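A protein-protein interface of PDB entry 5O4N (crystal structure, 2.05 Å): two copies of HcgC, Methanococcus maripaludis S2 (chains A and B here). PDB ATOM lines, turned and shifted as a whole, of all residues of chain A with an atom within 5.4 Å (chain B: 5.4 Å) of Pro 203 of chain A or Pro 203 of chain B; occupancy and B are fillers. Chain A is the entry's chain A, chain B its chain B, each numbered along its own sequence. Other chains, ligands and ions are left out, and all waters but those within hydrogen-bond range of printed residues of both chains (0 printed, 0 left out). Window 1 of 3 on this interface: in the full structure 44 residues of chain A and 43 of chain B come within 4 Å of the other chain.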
ATOM      1  N   ILE A 185      -6.584  18.179   7.876  1.00  0.00           N
ATOM      2  CA  ILE A 185      -7.605  18.933   8.623  1.00  0.00           C
ATOM      3  C   ILE A 185      -7.417  20.428   8.439  1.00  0.00           C
ATOM      4  O   ILE A 185      -8.391  21.125   8.133  1.00  0.00           O
ATOM      5  CB  ILE A 185      -7.689  18.488  10.122  1.00  0.00           C
ATOM      6  CG1 ILE A 185      -8.189  17.055  10.214  1.00  0.00           C
ATOM      7  CG2 ILE A 185      -8.595  19.431  10.964  1.00  0.00           C
ATOM      8  CD1 ILE A 185      -8.058  16.380  11.586  1.00  0.00           C
ATOM      9  N   MET A 186      -6.201  20.913   8.624  1.00  0.00           N
ATOM     10  CA  MET A 186      -5.870  22.338   8.481  1.00  0.00           C
ATOM     11  C   MET A 186      -6.163  22.843   7.084  1.00  0.00           C
ATOM     12  O   MET A 186      -6.765  23.902   6.952  1.00  0.00           O
ATOM     13  CB  MET A 186      -4.403  22.595   8.861  1.00  0.00           C
ATOM     14  CG  MET A 186      -4.120  22.384  10.355  1.00  0.00           C
ATOM     15  SD  MET A 186      -5.035  23.481  11.438  1.00  0.00           S
ATOM     16  CE  MET A 186      -4.115  25.062  11.150  1.00  0.00           C
ATOM     17  N   CYS A 189      -9.963  23.009   6.577  1.00  0.00           N
ATOM     18  CA  CYS A 189     -10.487  24.200   7.283  1.00  0.00           C
ATOM     19  C   CYS A 189     -10.350  25.457   6.487  1.00  0.00           C
ATOM     20  O   CYS A 189     -11.273  26.262   6.468  1.00  0.00           O
ATOM     21  CB  CYS A 189      -9.806  24.392   8.634  1.00  0.00           C
ATOM     22  SG  CYS A 189     -10.421  23.314   9.909  1.00  0.00           S
ATOM     23  N   THR A 201     -14.558  28.257  11.199  1.00  0.00           N
ATOM     24  CA  THR A 201     -14.281  26.829  11.117  1.00  0.00           C
ATOM     25  C   THR A 201     -13.296  26.406  12.161  1.00  0.00           C
ATOM     26  O   THR A 201     -12.219  26.997  12.278  1.00  0.00           O
ATOM     27  CB  THR A 201     -13.745  26.501   9.705  1.00  0.00           C
ATOM     28  OG1 THR A 201     -14.608  27.083   8.729  1.00  0.00           O
ATOM     29  CG2 THR A 201     -13.676  25.000   9.441  1.00  0.00           C
ATOM     30  N   ILE A 202     -13.653  25.388  12.924  1.00  0.00           N
ATOM     31  CA  ILE A 202     -12.820  24.871  13.982  1.00  0.00           C
ATOM     32  C   ILE A 202     -12.220  23.505  13.693  1.00  0.00           C
ATOM     33  O   ILE A 202     -12.973  22.533  13.582  1.00  0.00           O
ATOM     34  CB  ILE A 202     -13.634  24.702  15.303  1.00  0.00           C
ATOM     35  CG1 ILE A 202     -14.283  26.004  15.790  1.00  0.00           C
ATOM     36  CG2 ILE A 202     -12.763  24.053  16.429  1.00  0.00           C
ATOM     37  CD1 ILE A 202     -13.360  27.044  16.309  1.00  0.00           C
ATOM     38  N   PRO A 203     -10.889  23.377  13.658  1.00  0.00           N
ATOM     39  CA  PRO A 203     -10.304  22.028  13.488  1.00  0.00           C
ATOM     40  C   PRO A 203     -10.276  21.492  14.939  1.00  0.00           C
ATOM     41  O   PRO A 203      -9.774  22.185  15.828  1.00  0.00           O
ATOM     42  CB  PRO A 203      -8.904  22.300  12.977  1.00  0.00           C
ATOM     43  CG  PRO A 203      -8.569  23.662  13.477  1.00  0.00           C
ATOM     44  CD  PRO A 203      -9.845  24.407  13.799  1.00  0.00           C
ATOM     45  N   ASN A 204     -10.798  20.308  15.202  1.00  0.00           N
ATOM     46  CA  ASN A 204     -10.821  19.736  16.562  1.00  0.00           C
ATOM     47  C   ASN A 204      -9.538  19.006  16.820  1.00  0.00           C
ATOM     48  O   ASN A 204      -9.485  17.791  16.825  1.00  0.00           O
ATOM     49  CB  ASN A 204     -12.035  18.852  16.742  1.00  0.00           C
ATOM     50  CG  ASN A 204     -13.314  19.649  16.657  1.00  0.00           C
ATOM     51  OD1 ASN A 204     -13.491  20.626  17.387  1.00  0.00           O
ATOM     52  ND2 ASN A 204     -14.216  19.286  15.751  1.00  0.00           N
ATOM     53  N   LEU A 205      -8.486  19.767  17.024  1.00  0.00           N
ATOM     54  CA  LEU A 205      -7.159  19.247  17.238  1.00  0.00           C
ATOM     55  C   LEU A 205      -6.610  19.597  18.573  1.00  0.00           C
ATOM     56  O   LEU A 205      -7.013  20.576  19.205  1.00  0.00           O
ATOM     57  CB  LEU A 205      -6.228  19.842  16.156  1.00  0.00           C
ATOM     58  CG  LEU A 205      -6.505  19.465  14.706  1.00  0.00           C
ATOM     59  CD1 LEU A 205      -5.692  20.361  13.756  1.00  0.00           C
ATOM     60  CD2 LEU A 205      -6.173  18.009  14.444  1.00  0.00           C
ATOM     61  N   LYS A 206      -5.666  18.774  18.991  1.00  0.00           N
ATOM     62  CA  LYS A 206      -4.929  18.917  20.242  1.00  0.00           C
ATOM     63  C   LYS A 206      -3.638  18.126  20.060  1.00  0.00           C
ATOM     64  O   LYS A 206      -3.478  17.412  19.050  1.00  0.00           O
ATOM     65  CB  LYS A 206      -5.733  18.417  21.453  1.00  0.00           C
ATOM     66  CG  LYS A 206      -6.081  16.943  21.427  1.00  0.00           C
ATOM     67  CD  LYS A 206      -6.555  16.442  22.777  1.00  0.00           C
ATOM     68  CE  LYS A 206      -5.409  16.174  23.740  1.00  0.00           C
ATOM     69  NZ  LYS A 206      -5.850  16.138  25.158  1.00  0.00           N
ATOM     70  N   ALA A 229     -13.685  15.658  12.891  1.00  0.00           N
ATOM     71  CA  ALA A 229     -12.490  16.370  12.476  1.00  0.00           C
ATOM     72  C   ALA A 229     -12.696  17.890  12.460  1.00  0.00           C
ATOM     73  O   ALA A 229     -11.802  18.637  12.869  1.00  0.00           O
ATOM     74  CB  ALA A 229     -12.058  15.876  11.108  1.00  0.00           C
ATOM     75  N   ILE A 230     -13.869  18.350  12.015  1.00  0.00           N
ATOM     76  CA  ILE A 230     -14.147  19.785  11.941  1.00  0.00           C
ATOM     77  C   ILE A 230     -15.527  20.163  12.428  1.00  0.00           C
ATOM     78  O   ILE A 230     -16.489  19.401  12.246  1.00  0.00           O
ATOM     79  CB  ILE A 230     -13.927  20.245  10.437  1.00  0.00           C
ATOM     80  CG1 ILE A 230     -12.430  20.182  10.026  1.00  0.00           C
ATOM     81  CG2 ILE A 230     -14.501  21.661  10.165  1.00  0.00           C
ATOM     82  CD1 ILE A 230     -12.164  20.329   8.553  1.00  0.00           C
ATOM     83  N   THR A 231     -15.635  21.366  13.021  1.00  0.00           N
ATOM     84  CA  THR A 231     -16.911  21.933  13.496  1.00  0.00           C
ATOM     85  C   THR A 231     -17.035  23.266  12.759  1.00  0.00           C
ATOM     86  O   THR A 231     -16.093  24.061  12.738  1.00  0.00           O
ATOM     87  CB  THR A 231     -17.035  22.000  15.016  1.00  0.00           C
ATOM     88  OG1 THR A 231     -16.908  20.666  15.518  1.00  0.00           O
ATOM     89  CG2 THR A 231     -18.393  22.575  15.453  1.00  0.00           C
ATOM     90  N   ILE B 185      -5.396  32.463  15.326  1.00  0.00           N
ATOM     91  CA  ILE B 185      -4.721  31.197  15.625  1.00  0.00           C
ATOM     92  C   ILE B 185      -4.429  30.421  14.352  1.00  0.00           C
ATOM     93  O   ILE B 185      -3.293  29.973  14.183  1.00  0.00           O
ATOM     94  CB  ILE B 185      -5.476  30.364  16.701  1.00  0.00           C
ATOM     95  CG1 ILE B 185      -5.440  31.086  18.049  1.00  0.00           C
ATOM     96  CG2 ILE B 185      -4.890  28.934  16.858  1.00  0.00           C
ATOM     97  CD1 ILE B 185      -6.368  30.542  19.141  1.00  0.00           C
ATOM     98  N   MET B 186      -5.438  30.271  13.470  1.00  0.00           N
ATOM     99  CA  MET B 186      -5.308  29.548  12.213  1.00  0.00           C
ATOM    100  C   MET B 186      -4.255  30.178  11.308  1.00  0.00           C
ATOM    101  O   MET B 186      -3.432  29.443  10.741  1.00  0.00           O
ATOM    102  CB  MET B 186      -6.680  29.437  11.508  1.00  0.00           C
ATOM    103  CG  MET B 186      -7.677  28.545  12.249  1.00  0.00           C
ATOM    104  SD  MET B 186      -7.146  26.838  12.379  1.00  0.00           S
ATOM    105  CE  MET B 186      -7.459  26.265  10.687  1.00  0.00           C
ATOM    106  N   CYS B 189      -0.782  29.539  12.776  1.00  0.00           N
ATOM    107  CA  CYS B 189      -0.393  28.149  12.495  1.00  0.00           C
ATOM    108  C   CYS B 189       0.177  27.972  11.110  1.00  0.00           C
ATOM    109  O   CYS B 189       1.152  27.252  10.933  1.00  0.00           O
ATOM    110  CB  CYS B 189      -1.572  27.198  12.680  1.00  0.00           C
ATOM    111  SG  CYS B 189      -1.923  26.806  14.379  1.00  0.00           S
ATOM    112  N   THR B 201       2.148  21.748  13.393  1.00  0.00           N
ATOM    113  CA  THR B 201       1.625  22.782  14.275  1.00  0.00           C
ATOM    114  C   THR B 201       0.185  22.521  14.616  1.00  0.00           C
ATOM    115  O   THR B 201      -0.634  22.330  13.728  1.00  0.00           O
ATOM    116  CB  THR B 201       1.763  24.158  13.563  1.00  0.00           C
ATOM    117  OG1 THR B 201       3.089  24.295  13.069  1.00  0.00           O
ATOM    118  CG2 THR B 201       1.465  25.318  14.496  1.00  0.00           C
ATOM    119  N   ILE B 202      -0.123  22.527  15.899  1.00  0.00           N
ATOM    120  CA  ILE B 202      -1.476  22.277  16.377  1.00  0.00           C
ATOM    121  C   ILE B 202      -2.164  23.491  16.947  1.00  0.00           C
ATOM    122  O   ILE B 202      -1.705  24.017  17.976  1.00  0.00           O
ATOM    123  CB  ILE B 202      -1.469  21.220  17.520  1.00  0.00           C
ATOM    124  CG1 ILE B 202      -0.843  19.878  17.103  1.00  0.00           C
ATOM    125  CG2 ILE B 202      -2.880  21.013  18.119  1.00  0.00           C
ATOM    126  CD1 ILE B 202      -1.603  19.059  16.163  1.00  0.00           C
ATOM    127  N   PRO B 203      -3.299  23.916  16.376  1.00  0.00           N
ATOM    128  CA  PRO B 203      -4.044  25.025  16.992  1.00  0.00           C
ATOM    129  C   PRO B 203      -4.893  24.308  18.067  1.00  0.00           C
ATOM    130  O   PRO B 203      -5.580  23.337  17.747  1.00  0.00           O
ATOM    131  CB  PRO B 203      -4.916  25.552  15.864  1.00  0.00           C
ATOM    132  CG  PRO B 203      -5.108  24.412  14.959  1.00  0.00           C
ATOM    133  CD  PRO B 203      -4.000  23.399  15.181  1.00  0.00           C
ATOM    134  N   ASN B 204      -4.858  24.749  19.322  1.00  0.00           N
ATOM    135  CA  ASN B 204      -5.634  24.094  20.398  1.00  0.00           C
ATOM    136  C   ASN B 204      -7.020  24.671  20.440  1.00  0.00           C
ATOM    137  O   ASN B 204      -7.368  25.429  21.316  1.00  0.00           O
ATOM    138  CB  ASN B 204      -4.903  24.236  21.728  1.00  0.00           C
ATOM    139  CG  ASN B 204      -3.598  23.502  21.719  1.00  0.00           C
ATOM    140  OD1 ASN B 204      -3.564  22.308  21.452  1.00  0.00           O
ATOM    141  ND2 ASN B 204      -2.492  24.185  21.973  1.00  0.00           N
ATOM    142  N   LEU B 205      -7.822  24.292  19.470  1.00  0.00           N
ATOM    143  CA  LEU B 205      -9.171  24.794  19.330  1.00  0.00           C
ATOM    144  C   LEU B 205     -10.206  23.735  19.457  1.00  0.00           C
ATOM    145  O   LEU B 205      -9.961  22.549  19.224  1.00  0.00           O
ATOM    146  CB  LEU B 205      -9.290  25.428  17.933  1.00  0.00           C
ATOM    147  CG  LEU B 205      -8.446  26.663  17.630  1.00  0.00           C
ATOM    148  CD1 LEU B 205      -8.464  26.982  16.142  1.00  0.00           C
ATOM    149  CD2 LEU B 205      -8.950  27.862  18.418  1.00  0.00           C
ATOM    150  N   LYS B 206     -11.384  24.190  19.832  1.00  0.00           N
ATOM    151  CA  LYS B 206     -12.580  23.370  19.982  1.00  0.00           C
ATOM    152  C   LYS B 206     -13.760  24.321  19.846  1.00  0.00           C
ATOM    153  O   LYS B 206     -13.573  25.550  19.806  1.00  0.00           O
ATOM    154  CB  LYS B 206     -12.604  22.605  21.321  1.00  0.00           C
ATOM    155  CG  LYS B 206     -12.645  23.498  22.568  1.00  0.00           C
ATOM    156  CD  LYS B 206     -13.018  22.731  23.805  1.00  0.00           C
ATOM    157  CE  LYS B 206     -14.516  22.472  23.911  1.00  0.00           C
ATOM    158  NZ  LYS B 206     -14.835  21.347  24.839  1.00  0.00           N
ATOM    159  N   ALA B 229      -2.446  28.680  23.006  1.00  0.00           N
ATOM    160  CA  ALA B 229      -3.077  28.824  21.714  1.00  0.00           C
ATOM    161  C   ALA B 229      -2.531  27.836  20.692  1.00  0.00           C
ATOM    162  O   ALA B 229      -3.310  27.279  19.885  1.00  0.00           O
ATOM    163  CB  ALA B 229      -2.902  30.247  21.207  1.00  0.00           C
ATOM    164  N   ILE B 230      -1.214  27.607  20.705  1.00  0.00           N
ATOM    165  CA  ILE B 230      -0.595  26.697  19.741  1.00  0.00           C
ATOM    166  C   ILE B 230       0.442  25.782  20.371  1.00  0.00           C
ATOM    167  O   ILE B 230       1.150  26.175  21.285  1.00  0.00           O
ATOM    168  CB  ILE B 230       0.052  27.560  18.579  1.00  0.00           C
ATOM    169  CG1 ILE B 230      -1.026  28.241  17.698  1.00  0.00           C
ATOM    170  CG2 ILE B 230       1.011  26.726  17.675  1.00  0.00           C
ATOM    171  CD1 ILE B 230      -0.504  29.291  16.753  1.00  0.00           C
ATOM    172  N   THR B 231       0.540  24.545  19.838  1.00  0.00           N
ATOM    173  CA  THR B 231       1.508  23.555  20.261  1.00  0.00           C
ATOM    174  C   THR B 231       2.287  23.222  18.990  1.00  0.00           C
ATOM    175  O   THR B 231       1.698  22.954  17.959  1.00  0.00           O
ATOM    176  CB  THR B 231       0.896  22.367  21.008  1.00  0.00           C
ATOM    177  OG1 THR B 231       0.259  22.891  22.181  1.00  0.00           O
ATOM    178  CG2 THR B 231       1.963  21.354  21.447  1.00  0.00           C
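O of Leu 205 of chain B sits close to O of Pro 203 of chain A (3.4 Å).
The backbone carbonyl oxygen of Leu 205 of chain A sits close to the backbone carbonyl oxygen of Pro 203 of chain B.
The side-chain sulfur of Cys 189 of chain A sits at hydrogen-bond distance from the backbone carbonyl oxygen of Ile 185 of chain A (3.5 Å).
The backbone NH of Ile 202 of chain A lies within hydrogen-bond range of the backbone carbonyl oxygen of Thr 231 of chain A, 2.8 Å away.
The side-chain hydroxyl (OG1) of Thr 231 of chain A sits at hydrogen-bond distance from the side-chain amide nitrogen (ND2) of Asn 204 of chain A (3.0 Å).
N of Ile 202 of chain B is in hydrogen-bond range of O of Thr 231 of chain B (2.8 Å).
N of Asn 204 of chain B is in hydrogen-bond range of O of Ala 229 of chain B (3.0 Å).
The side-chain amide nitrogen of Asn 204 of chain B sits at hydrogen-bond distance from the side-chain hydroxyl of Thr 231 of chain B, at 3.0 Å.
Met 186 of chain B touches Met 186 of chain A.
Met 186 of chain B touches Cys 189 of chain A.
Lys 206 of chain B touches Ile 202 of chain A (C to CG2, 3.6 Å).
Pro 203 of chain A touches Met 186 of chain B (CG to SD, 3.6 Å).
O of Leu 205 of chain B touches CA of Asn 204 of chain A (3.97 Å).
Lys 206 of chain B touches Asn 204 of chain A (CA to OD1, 3.9 Å).
Asn 204 of chain B touches Leu 205 of chain A (CA to O, 3.96 Å).
O of Leu 205 of chain A touches O of Leu 205 of chain B, at 3.5 Å.
Lys 206 of chain A touches Ile 202 of chain B (C to CG2, 3.6 Å).
Asn 204 of chain B touches Lys 206 of chain A.
Of the printed residues of chain B, Ile 202 of chain A touches Leu 205 (3.98 Å) and Lys 206 (3.6 Å).
Pro 203 of chain A touches just these residues of chain B: Met 186 (3.6 Å), Pro 203 (3.8 Å) and Leu 205 (3.4 Å).
Of the printed residues of chain A, Pro 203 of chain B touches Met 186 (3.6 Å), Pro 203 (3.8 Å) and Leu 205 (3.4 Å).
Of the printed residues of chain A, Leu 205 of chain B touches Ile 202, Pro 203, Asn 204 and Leu 205.
The nearest residue of chain A that does not touch Pro 203 of chain B is Lys 206 of chain A (4.7 Å).
Of the 12 printed residues of chain A, 7 touch a printed residue of chain B.
Of the 12 printed residues of chain B, 7 touch a printed residue of chain A.
Hydrophobic or aromatic side chains of chain B within 4 Å of the printed part of chain A: Met 186, Ile 202, Pro 203 and Leu 205.
Among the printed residues, 16 pairs touch across the chains.
Among the printed residues, no Asp or Glu carboxylate lies within 4 Å of a Lys or Arg side-chain nitrogen of the other chain.
Met 186 of chain B touches its own counterpart, Met 186 of chain A.
Ile 202 of chain A touches Lys 206 of chain B, and with the chains exchanged Lys 206 of chain A touches Ile 202 of chain B.
Pro 203 of chain A touches Leu 205 of chain B, and with the chains exchanged Leu 205 of chain A touches Pro 203 of chain B.
Asn 204 of chain A touches Lys 206 of chain B, and with the chains exchanged Lys 206 of chain A touches Asn 204 of chain B.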
